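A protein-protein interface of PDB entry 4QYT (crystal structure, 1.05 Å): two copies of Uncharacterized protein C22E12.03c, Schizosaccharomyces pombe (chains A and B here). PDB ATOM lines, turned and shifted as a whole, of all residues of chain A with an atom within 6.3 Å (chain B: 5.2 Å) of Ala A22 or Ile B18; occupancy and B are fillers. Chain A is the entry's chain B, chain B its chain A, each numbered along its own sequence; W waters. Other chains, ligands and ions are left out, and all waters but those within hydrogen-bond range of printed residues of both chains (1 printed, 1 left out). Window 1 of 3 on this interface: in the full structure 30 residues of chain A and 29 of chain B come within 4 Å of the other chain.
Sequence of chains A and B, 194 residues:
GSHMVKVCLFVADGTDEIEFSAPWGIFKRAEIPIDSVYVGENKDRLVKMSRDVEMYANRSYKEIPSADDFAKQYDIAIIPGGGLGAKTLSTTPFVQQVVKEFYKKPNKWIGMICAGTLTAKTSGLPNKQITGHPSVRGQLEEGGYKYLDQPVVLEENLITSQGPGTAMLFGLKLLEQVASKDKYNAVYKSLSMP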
ATOM      1  N   GLU A  17     -28.924  12.417  -9.656  1.00  0.00           N
ATOM      2  CA  GLU A  17     -29.031  11.267 -10.553  1.00  0.00           C
ATOM      3  C   GLU A  17     -27.681  10.859 -11.134  1.00  0.00           C
ATOM      4  O   GLU A  17     -27.399   9.668 -11.297  1.00  0.00           O
ATOM      5  CB  GLU A  17     -29.973  11.604 -11.715  1.00  0.00           C
ATOM      6  CG  GLU A  17     -31.443  11.822 -11.382  1.00  0.00           C
ATOM      7  CD  GLU A  17     -31.868  13.201 -10.906  1.00  0.00           C
ATOM      8  OE1 GLU A  17     -31.010  14.010 -10.488  1.00  0.00           O
ATOM      9  OE2 GLU A  17     -33.084  13.464 -10.987  1.00  0.00           O
ATOM     10  N   ILE A  18     -26.863  11.833 -11.530  1.00  0.00           N
ATOM     11  CA  ILE A  18     -25.575  11.542 -12.175  1.00  0.00           C
ATOM     12  C   ILE A  18     -24.646  10.855 -11.178  1.00  0.00           C
ATOM     13  O   ILE A  18     -23.979   9.851 -11.499  1.00  0.00           O
ATOM     14  CB  ILE A  18     -24.975  12.819 -12.774  1.00  0.00           C
ATOM     15  CG1 ILE A  18     -25.852  13.310 -13.928  1.00  0.00           C
ATOM     16  CG2 ILE A  18     -23.537  12.581 -13.222  1.00  0.00           C
ATOM     17  CD1 ILE A  18     -25.584  14.738 -14.335  1.00  0.00           C
ATOM     18  N   GLU A  19     -24.571  11.400  -9.977  1.00  0.00           N
ATOM     19  CA  GLU A  19     -23.700  10.848  -8.944  1.00  0.00           C
ATOM     20  C   GLU A  19     -24.140   9.500  -8.419  1.00  0.00           C
ATOM     21  O   GLU A  19     -23.307   8.734  -7.999  1.00  0.00           O
ATOM     22  CB  GLU A  19     -23.560  11.853  -7.826  1.00  0.00           C
ATOM     23  CG  GLU A  19     -22.835  13.091  -8.307  1.00  0.00           C
ATOM     24  CD  GLU A  19     -23.007  14.298  -7.466  1.00  0.00           C
ATOM     25  OE1 GLU A  19     -23.516  14.218  -6.371  1.00  0.00           O
ATOM     26  OE2 GLU A  19     -22.602  15.401  -7.942  1.00  0.00           O
ATOM     27  N   PHE A  20     -25.438   9.214  -8.442  1.00  0.00           N
ATOM     28  CA  PHE A  20     -25.912   7.864  -8.190  1.00  0.00           C
ATOM     29  C   PHE A  20     -25.505   6.915  -9.314  1.00  0.00           C
ATOM     30  O   PHE A  20     -24.975   5.824  -9.085  1.00  0.00           O
ATOM     31  CB  PHE A  20     -27.425   7.897  -7.973  1.00  0.00           C
ATOM     32  CG  PHE A  20     -28.026   6.549  -7.689  1.00  0.00           C
ATOM     33  CD1 PHE A  20     -28.307   5.668  -8.700  1.00  0.00           C
ATOM     34  CD2 PHE A  20     -28.313   6.147  -6.374  1.00  0.00           C
ATOM     35  CE1 PHE A  20     -28.815   4.381  -8.432  1.00  0.00           C
ATOM     36  CE2 PHE A  20     -28.825   4.906  -6.103  1.00  0.00           C
ATOM     37  CZ  PHE A  20     -29.061   4.027  -7.121  1.00  0.00           C
ATOM     38  N   SER A  21     -25.845   7.296 -10.542  1.00  0.00           N
ATOM     39  CA  SER A  21     -25.731   6.341 -11.640  1.00  0.00           C
ATOM     40  C   SER A  21     -24.304   5.904 -11.948  1.00  0.00           C
ATOM     41  O   SER A  21     -24.099   4.775 -12.417  1.00  0.00           O
ATOM     42  CB  SER A  21     -26.414   6.898 -12.887  1.00  0.00           C
ATOM     43  OG  SER A  21     -27.793   7.143 -12.654  1.00  0.00           O
ATOM     44  N   ALA A  22     -23.317   6.782 -11.785  1.00  0.00           N
ATOM     45  CA  ALA A  22     -21.951   6.423 -12.171  1.00  0.00           C
ATOM     46  C   ALA A  22     -21.414   5.246 -11.332  1.00  0.00           C
ATOM     47  O   ALA A  22     -21.064   4.207 -11.876  1.00  0.00           O
ATOM     48  CB  ALA A  22     -21.064   7.644 -12.122  1.00  0.00           C
ATOM     49  N   PRO A  23     -21.363   5.362  -9.997  1.00  0.00           N
ATOM     50  CA  PRO A  23     -20.906   4.194  -9.225  1.00  0.00           C
ATOM     51  C   PRO A  23     -21.820   2.993  -9.399  1.00  0.00           C
ATOM     52  O   PRO A  23     -21.351   1.857  -9.425  1.00  0.00           O
ATOM     53  CB  PRO A  23     -20.889   4.704  -7.779  1.00  0.00           C
ATOM     54  CG  PRO A  23     -21.791   5.898  -7.771  1.00  0.00           C
ATOM     55  CD  PRO A  23     -21.590   6.512  -9.121  1.00  0.00           C
ATOM     56  N   TRP A  24     -23.136   3.220  -9.505  1.00  0.00           N
ATOM     57  CA  TRP A  24     -24.040   2.117  -9.735  1.00  0.00           C
ATOM     58  C   TRP A  24     -23.632   1.315 -10.972  1.00  0.00           C
ATOM     59  O   TRP A  24     -23.463   0.111 -10.942  1.00  0.00           O
ATOM     60  CB  TRP A  24     -25.468   2.643  -9.885  1.00  0.00           C
ATOM     61  CG  TRP A  24     -26.462   1.562 -10.097  1.00  0.00           C
ATOM     62  CD1 TRP A  24     -26.906   1.078 -11.285  1.00  0.00           C
ATOM     63  CD2 TRP A  24     -27.101   0.750  -9.083  1.00  0.00           C
ATOM     64  NE1 TRP A  24     -27.768   0.023 -11.075  1.00  0.00           N
ATOM     65  CE2 TRP A  24     -27.918  -0.169  -9.735  1.00  0.00           C
ATOM     66  CE3 TRP A  24     -27.082   0.756  -7.693  1.00  0.00           C
ATOM     67  CZ2 TRP A  24     -28.704  -1.083  -9.052  1.00  0.00           C
ATOM     68  CZ3 TRP A  24     -27.864  -0.164  -7.019  1.00  0.00           C
ATOM     69  CH2 TRP A  24     -28.651  -1.053  -7.692  1.00  0.00           C
ATOM     70  N   GLY A  25     -23.508   2.013 -12.103  1.00  0.00           N
ATOM     71  CA  GLY A  25     -23.195   1.339 -13.347  1.00  0.00           C
ATOM     72  C   GLY A  25     -21.807   0.734 -13.386  1.00  0.00           C
ATOM     73  O   GLY A  25     -21.595  -0.271 -14.059  1.00  0.00           O
ATOM     74  N   ILE A  26     -20.866   1.364 -12.700  1.00  0.00           N
ATOM     75  CA  ILE A  26     -19.493   0.845 -12.664  1.00  0.00           C
ATOM     76  C   ILE A  26     -19.435  -0.458 -11.866  1.00  0.00           C
ATOM     77  O   ILE A  26     -18.863  -1.455 -12.331  1.00  0.00           O
ATOM     78  CB  ILE A  26     -18.540   1.926 -12.144  1.00  0.00           C
ATOM     79  CG1 ILE A  26     -18.392   3.030 -13.213  1.00  0.00           C
ATOM     80  CG2 ILE A  26     -17.197   1.333 -11.790  1.00  0.00           C
ATOM     81  CD1 ILE A  26     -17.742   4.299 -12.696  1.00  0.00           C
ATOM     82  N   PHE A  27     -20.054  -0.489 -10.681  1.00  0.00           N
ATOM     83  CA  PHE A  27     -20.045  -1.727  -9.892  1.00  0.00           C
ATOM     84  C   PHE A  27     -20.849  -2.820 -10.562  1.00  0.00           C
ATOM     85  O   PHE A  27     -20.453  -3.992 -10.508  1.00  0.00           O
ATOM     86  CB  PHE A  27     -20.430  -1.483  -8.437  1.00  0.00           C
ATOM     87  CG  PHE A  27     -19.290  -0.879  -7.639  1.00  0.00           C
ATOM     88  CD1 PHE A  27     -18.242  -1.694  -7.210  1.00  0.00           C
ATOM     89  CD2 PHE A  27     -19.236   0.460  -7.290  1.00  0.00           C
ATOM     90  CE1 PHE A  27     -17.175  -1.199  -6.496  1.00  0.00           C
ATOM     91  CE2 PHE A  27     -18.142   0.955  -6.603  1.00  0.00           C
ATOM     92  CZ  PHE A  27     -17.102   0.130  -6.215  1.00  0.00           C
ATOM     93  N   ARG A  29     -21.155  -3.262 -13.827  1.00  0.00           N
ATOM     94  CA  ARG A  29     -20.276  -3.803 -14.882  1.00  0.00           C
ATOM     95  C   ARG A  29     -19.156  -4.686 -14.321  1.00  0.00           C
ATOM     96  O   ARG A  29     -18.770  -5.664 -14.938  1.00  0.00           O
ATOM     97  CB  ARG A  29     -19.661  -2.643 -15.652  1.00  0.00           C
ATOM     98  CG  ARG A  29     -20.600  -1.981 -16.648  1.00  0.00           C
ATOM     99  CD  ARG A  29     -20.053  -0.661 -17.137  1.00  0.00           C
ATOM    100  NE  ARG A  29     -20.892  -0.060 -18.174  1.00  0.00           N
ATOM    101  CZ  ARG A  29     -22.046   0.572 -17.962  1.00  0.00           C
ATOM    102  NH1 ARG A  29     -22.554   0.696 -16.756  1.00  0.00           N
ATOM    103  NH2 ARG A  29     -22.688   1.036 -19.010  1.00  0.00           N
ATOM    104  N   ALA A 167     -18.094  12.119 -11.388  1.00  0.00           N
ATOM    105  CA  ALA A 167     -18.734  10.931 -10.832  1.00  0.00           C
ATOM    106  C   ALA A 167     -18.147   9.642 -11.393  1.00  0.00           C
ATOM    107  O   ALA A 167     -18.036   8.642 -10.649  1.00  0.00           O
ATOM    108  CB  ALA A 167     -20.239  11.004 -10.984  1.00  0.00           C
ATOM    109  N   MET A 168     -17.831   9.620 -12.687  1.00  0.00           N
ATOM    110  CA  MET A 168     -17.212   8.446 -13.259  1.00  0.00           C
ATOM    111  C   MET A 168     -15.833   8.188 -12.669  1.00  0.00           C
ATOM    112  O   MET A 168     -15.496   7.064 -12.307  1.00  0.00           O
ATOM    113  CB  MET A 168     -17.164   8.538 -14.766  1.00  0.00           C
ATOM    114  CG  MET A 168     -18.544   8.497 -15.422  1.00  0.00           C
ATOM    115  SD  MET A 168     -19.426   6.948 -15.255  1.00  0.00           S
ATOM    116  CE  MET A 168     -18.474   5.932 -16.366  1.00  0.00           C
ATOM    117  N   LEU A 169     -15.009   9.220 -12.571  1.00  0.00           N
ATOM    118  CA  LEU A 169     -13.689   9.060 -11.964  1.00  0.00           C
ATOM    119  C   LEU A 169     -13.818   8.601 -10.509  1.00  0.00           C
ATOM    120  O   LEU A 169     -13.025   7.780 -10.035  1.00  0.00           O
ATOM    121  CB  LEU A 169     -12.934  10.388 -12.015  1.00  0.00           C
ATOM    122  CG  LEU A 169     -12.557  10.830 -13.422  1.00  0.00           C
ATOM    123  CD1 LEU A 169     -12.116  12.266 -13.398  1.00  0.00           C
ATOM    124  CD2 LEU A 169     -11.462   9.930 -13.966  1.00  0.00           C
ATOM    125  N   GLY A 171     -16.389   6.793  -9.137  1.00  0.00           N
ATOM    126  CA  GLY A 171     -16.735   5.394  -9.107  1.00  0.00           C
ATOM    127  C   GLY A 171     -15.574   4.489  -9.449  1.00  0.00           C
ATOM    128  O   GLY A 171     -15.402   3.421  -8.830  1.00  0.00           O
ATOM    129  N   LEU A 191     -15.908   1.634 -20.633  1.00  0.00           N
ATOM    130  CA  LEU A 191     -16.606   2.888 -20.381  1.00  0.00           C
ATOM    131  C   LEU A 191     -16.401   3.927 -21.471  1.00  0.00           C
ATOM    132  O   LEU A 191     -17.162   4.883 -21.553  1.00  0.00           O
ATOM    133  CB  LEU A 191     -16.168   3.446 -19.048  1.00  0.00           C
ATOM    134  CG  LEU A 191     -16.435   2.545 -17.859  1.00  0.00           C
ATOM    135  CD1 LEU A 191     -15.850   3.142 -16.614  1.00  0.00           C
ATOM    136  CD2 LEU A 191     -17.891   2.212 -17.676  1.00  0.00           C
ATOM    137  N   ASP B  16     -29.254   2.428 -20.624  1.00  0.00           N
ATOM    138  CA  ASP B  16     -28.183   2.655 -19.668  1.00  0.00           C
ATOM    139  C   ASP B  16     -28.457   3.824 -18.716  1.00  0.00           C
ATOM    140  O   ASP B  16     -28.774   4.929 -19.154  1.00  0.00           O
ATOM    141  CB  ASP B  16     -26.879   2.912 -20.426  1.00  0.00           C
ATOM    142  CG  ASP B  16     -25.734   3.058 -19.491  1.00  0.00           C
ATOM    143  OD1 ASP B  16     -25.326   2.013 -18.941  1.00  0.00           O
ATOM    144  OD2 ASP B  16     -25.250   4.192 -19.306  1.00  0.00           O
ATOM    145  N   GLU B  17     -28.248   3.565 -17.437  1.00  0.00           N
ATOM    146  CA  GLU B  17     -28.503   4.575 -16.403  1.00  0.00           C
ATOM    147  C   GLU B  17     -27.598   5.796 -16.537  1.00  0.00           C
ATOM    148  O   GLU B  17     -28.045   6.942 -16.319  1.00  0.00           O
ATOM    149  CB  GLU B  17     -28.309   3.982 -15.016  1.00  0.00           C
ATOM    150  CG  GLU B  17     -29.289   2.892 -14.594  1.00  0.00           C
ATOM    151  CD  GLU B  17     -28.956   1.467 -14.994  1.00  0.00           C
ATOM    152  OE1 GLU B  17     -28.152   1.255 -15.955  1.00  0.00           O
ATOM    153  OE2 GLU B  17     -29.518   0.557 -14.369  1.00  0.00           O
ATOM    154  N   ILE B  18     -26.321   5.581 -16.828  1.00  0.00           N
ATOM    155  CA  ILE B  18     -25.367   6.680 -16.895  1.00  0.00           C
ATOM    156  C   ILE B  18     -25.691   7.591 -18.078  1.00  0.00           C
ATOM    157  O   ILE B  18     -25.686   8.837 -17.951  1.00  0.00           O
ATOM    158  CB  ILE B  18     -23.923   6.146 -16.936  1.00  0.00           C
ATOM    159  CG1 ILE B  18     -23.594   5.458 -15.617  1.00  0.00           C
ATOM    160  CG2 ILE B  18     -22.955   7.262 -17.260  1.00  0.00           C
ATOM    161  CD1 ILE B  18     -22.345   4.568 -15.675  1.00  0.00           C
ATOM    162  N   GLU B  19     -25.951   6.973 -19.218  1.00  0.00           N
ATOM    163  CA  GLU B  19     -26.234   7.734 -20.441  1.00  0.00           C
ATOM    164  C   GLU B  19     -27.576   8.449 -20.382  1.00  0.00           C
ATOM    165  O   GLU B  19     -27.722   9.488 -21.011  1.00  0.00           O
ATOM    166  CB  GLU B  19     -26.146   6.819 -21.626  1.00  0.00           C
ATOM    167  CG  GLU B  19     -24.723   6.336 -21.836  1.00  0.00           C
ATOM    168  CD  GLU B  19     -24.606   5.135 -22.679  1.00  0.00           C
ATOM    169  OE1 GLU B  19     -25.559   4.653 -23.265  1.00  0.00           O
ATOM    170  OE2 GLU B  19     -23.446   4.610 -22.679  1.00  0.00           O
ATOM    171  N   PHE B  20     -28.537   7.902 -19.643  1.00  0.00           N
ATOM    172  CA  PHE B  20     -29.784   8.612 -19.359  1.00  0.00           C
ATOM    173  C   PHE B  20     -29.526   9.815 -18.435  1.00  0.00           C
ATOM    174  O   PHE B  20     -29.947  10.927 -18.715  1.00  0.00           O
ATOM    175  CB  PHE B  20     -30.812   7.652 -18.731  1.00  0.00           C
ATOM    176  CG  PHE B  20     -32.142   8.310 -18.407  1.00  0.00           C
ATOM    177  CD1 PHE B  20     -32.275   9.132 -17.273  1.00  0.00           C
ATOM    178  CD2 PHE B  20     -33.225   8.196 -19.269  1.00  0.00           C
ATOM    179  CE1 PHE B  20     -33.473   9.779 -16.990  1.00  0.00           C
ATOM    180  CE2 PHE B  20     -34.405   8.840 -19.005  1.00  0.00           C
ATOM    181  CZ  PHE B  20     -34.511   9.650 -17.882  1.00  0.00           C
ATOM    182  N   SER B  21     -28.840   9.577 -17.308  1.00  0.00           N
ATOM    183  CA  SER B  21     -28.775  10.606 -16.262  1.00  0.00           C
ATOM    184  C   SER B  21     -27.987  11.851 -16.647  1.00  0.00           C
ATOM    185  O   SER B  21     -28.266  12.929 -16.136  1.00  0.00           O
ATOM    186  CB  SER B  21     -28.212   9.994 -14.974  1.00  0.00           C
ATOM    187  OG  SER B  21     -29.018   8.917 -14.507  1.00  0.00           O
ATOM    188  N   ALA B  22     -26.938  11.705 -17.454  1.00  0.00           N
ATOM    189  CA  ALA B  22     -26.121  12.870 -17.763  1.00  0.00           C
ATOM    190  C   ALA B  22     -26.900  13.950 -18.539  1.00  0.00           C
ATOM    191  O   ALA B  22     -27.009  15.084 -18.045  1.00  0.00           O
ATOM    192  CB  ALA B  22     -24.832  12.449 -18.467  1.00  0.00           C
ATOM    193  N   PRO B  23     -27.456  13.652 -19.730  1.00  0.00           N
ATOM    194  CA  PRO B  23     -28.259  14.678 -20.398  1.00  0.00           C
ATOM    195  C   PRO B  23     -29.421  15.128 -19.533  1.00  0.00           C
ATOM    196  O   PRO B  23     -29.783  16.305 -19.557  1.00  0.00           O
ATOM    197  CB  PRO B  23     -28.671  14.013 -21.715  1.00  0.00           C
ATOM    198  CG  PRO B  23     -28.527  12.524 -21.483  1.00  0.00           C
ATOM    199  CD  PRO B  23     -27.358  12.427 -20.545  1.00  0.00           C
ATOM    200  N   PRO B 164     -20.550   5.403 -21.640  1.00  0.00           N
ATOM    201  CA  PRO B 164     -20.880   6.015 -20.358  1.00  0.00           C
ATOM    202  C   PRO B 164     -19.896   7.067 -19.957  1.00  0.00           C
ATOM    203  O   PRO B 164     -20.280   8.089 -19.422  1.00  0.00           O
ATOM    204  CB  PRO B 164     -20.902   4.825 -19.388  1.00  0.00           C
ATOM    205  CG  PRO B 164     -20.897   3.633 -20.211  1.00  0.00           C
ATOM    206  CD  PRO B 164     -20.503   3.933 -21.592  1.00  0.00           C
ATOM    207  N   ALA B 167     -20.804  10.484 -21.501  1.00  0.00           N
ATOM    208  CA  ALA B 167     -22.182  10.959 -21.403  1.00  0.00           C
ATOM    209  C   ALA B 167     -22.274  12.418 -20.980  1.00  0.00           C
ATOM    210  O   ALA B 167     -23.148  13.147 -21.462  1.00  0.00           O
ATOM    211  CB  ALA B 167     -22.967  10.060 -20.505  1.00  0.00           C
HETATM  212  O   HOH W   1     -25.217   2.083 -16.219  1.00  0.00           O
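Ala A22 touches just one residue of chain B: Ile B18 (3.9 Å). Of the printed residues of chain A, Ile B18 touches Ser A21, Ala A22 and Met A168. Of the printed residues of chain B, Met A168 touches Ile B18 (3.8 Å). Printed residues of chain B within 4 Å of Ser A21: Glu B17 (3.7 Å), Ile B18 (3.3 Å) and Ser B21 (2.8 Å). Glu B19 touches none of the printed residues of chain A. Glu A19 touches none of the printed residues of chain B. The nearest printed residue of chain A that does not touch Ile B18 is Arg A29 (4.03 Å). The nearest printed residue of chain B that does not touch Trp A24 is Ile B18 (5.9 Å).
Hydrophobic or aromatic side chains of chain A within 4 Å of the printed part of chain B: Ile A18, Trp A24 and Met A168. Of the 10 printed residues of chain B, 6 touch a printed residue of chain A. Hydrophobic or aromatic side chains of chain B within 4 Å of the printed part of chain A: Ile B18 and Pro B164. Among the printed residues, 12 pairs touch across the chains. Among the printed residues, Asp or Glu carboxylates within 4 Å of a Lys or Arg side-chain nitrogen of the other chain: Arg A29 with Asp B16 (2.8 Å).
Water W1 lies within hydrogen-bond range of the side-chain carboxylate of Asp B16 (2.7 Å), the guanidinium group of Arg A29 (3.1 Å) and the side-chain carboxylate of Glu B17 (3.1 Å).
OD1 of Asp B16 lies within salt-bridge range of NH2 of Arg A29 (2.8 Å). The side-chain hydroxyl (OG) of Ser B21 sits at hydrogen-bond distance from the side-chain hydroxyl (OG) of Ser A21 (2.8 Å). N of Pro B164 lies close to O of Leu A191 (3.4 Å).
Glu A17 touches Ser B21, and with the chains exchanged Ser A21 touches Glu B17. Ile A18 touches Ser B21, and with the chains exchanged Ser A21 touches Ile B18. Ile A18 touches Ala B22, and with the chains exchanged Ala A22 touches Ile B18. Ser A21 touches its own counterpart, Ser B21. Positions printed for both chains: 17, 18, 19, 20, 21, 22, 23 and 167. Of the 12 pairs that touch across the chains among the printed residues, 7 have their exchanged pair printed and touching as well.
The backbone NH (N) of Ile B18 sits at hydrogen-bond distance from the side-chain carboxylate (OD2) of Asp B16 (3.0 Å). The side-chain carboxylate of Asp B16 is in hydrogen-bond range of the backbone NH of Glu B19, 2.9 Å away. O of Glu B17 sits at hydrogen-bond distance from OG of Ser B21, at 2.9 Å. OG of Ser A21 lies within hydrogen-bond range of O of Glu A17 (2.9 Å). O of Gly A25 lies within hydrogen-bond range of NH1 of Arg A29.
Among the printed residues, merely in contact across the chains: Glu A17 with Ser B21 (3.7 Å), Ile A18 with Ser B21 (3.3 Å), Ile A18 with Ala B22 (3.9 Å), Ser A21 with Glu B17 (3.7 Å), Ser A21 with Ile B18 (3.3 Å), Ala A22 with Ile B18 (3.9 Å), Trp A24 with Glu B17 (3.8 Å), Arg A29 with Pro B164 (3.4 Å) and Met A168 with Ile B18 (3.8 Å).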
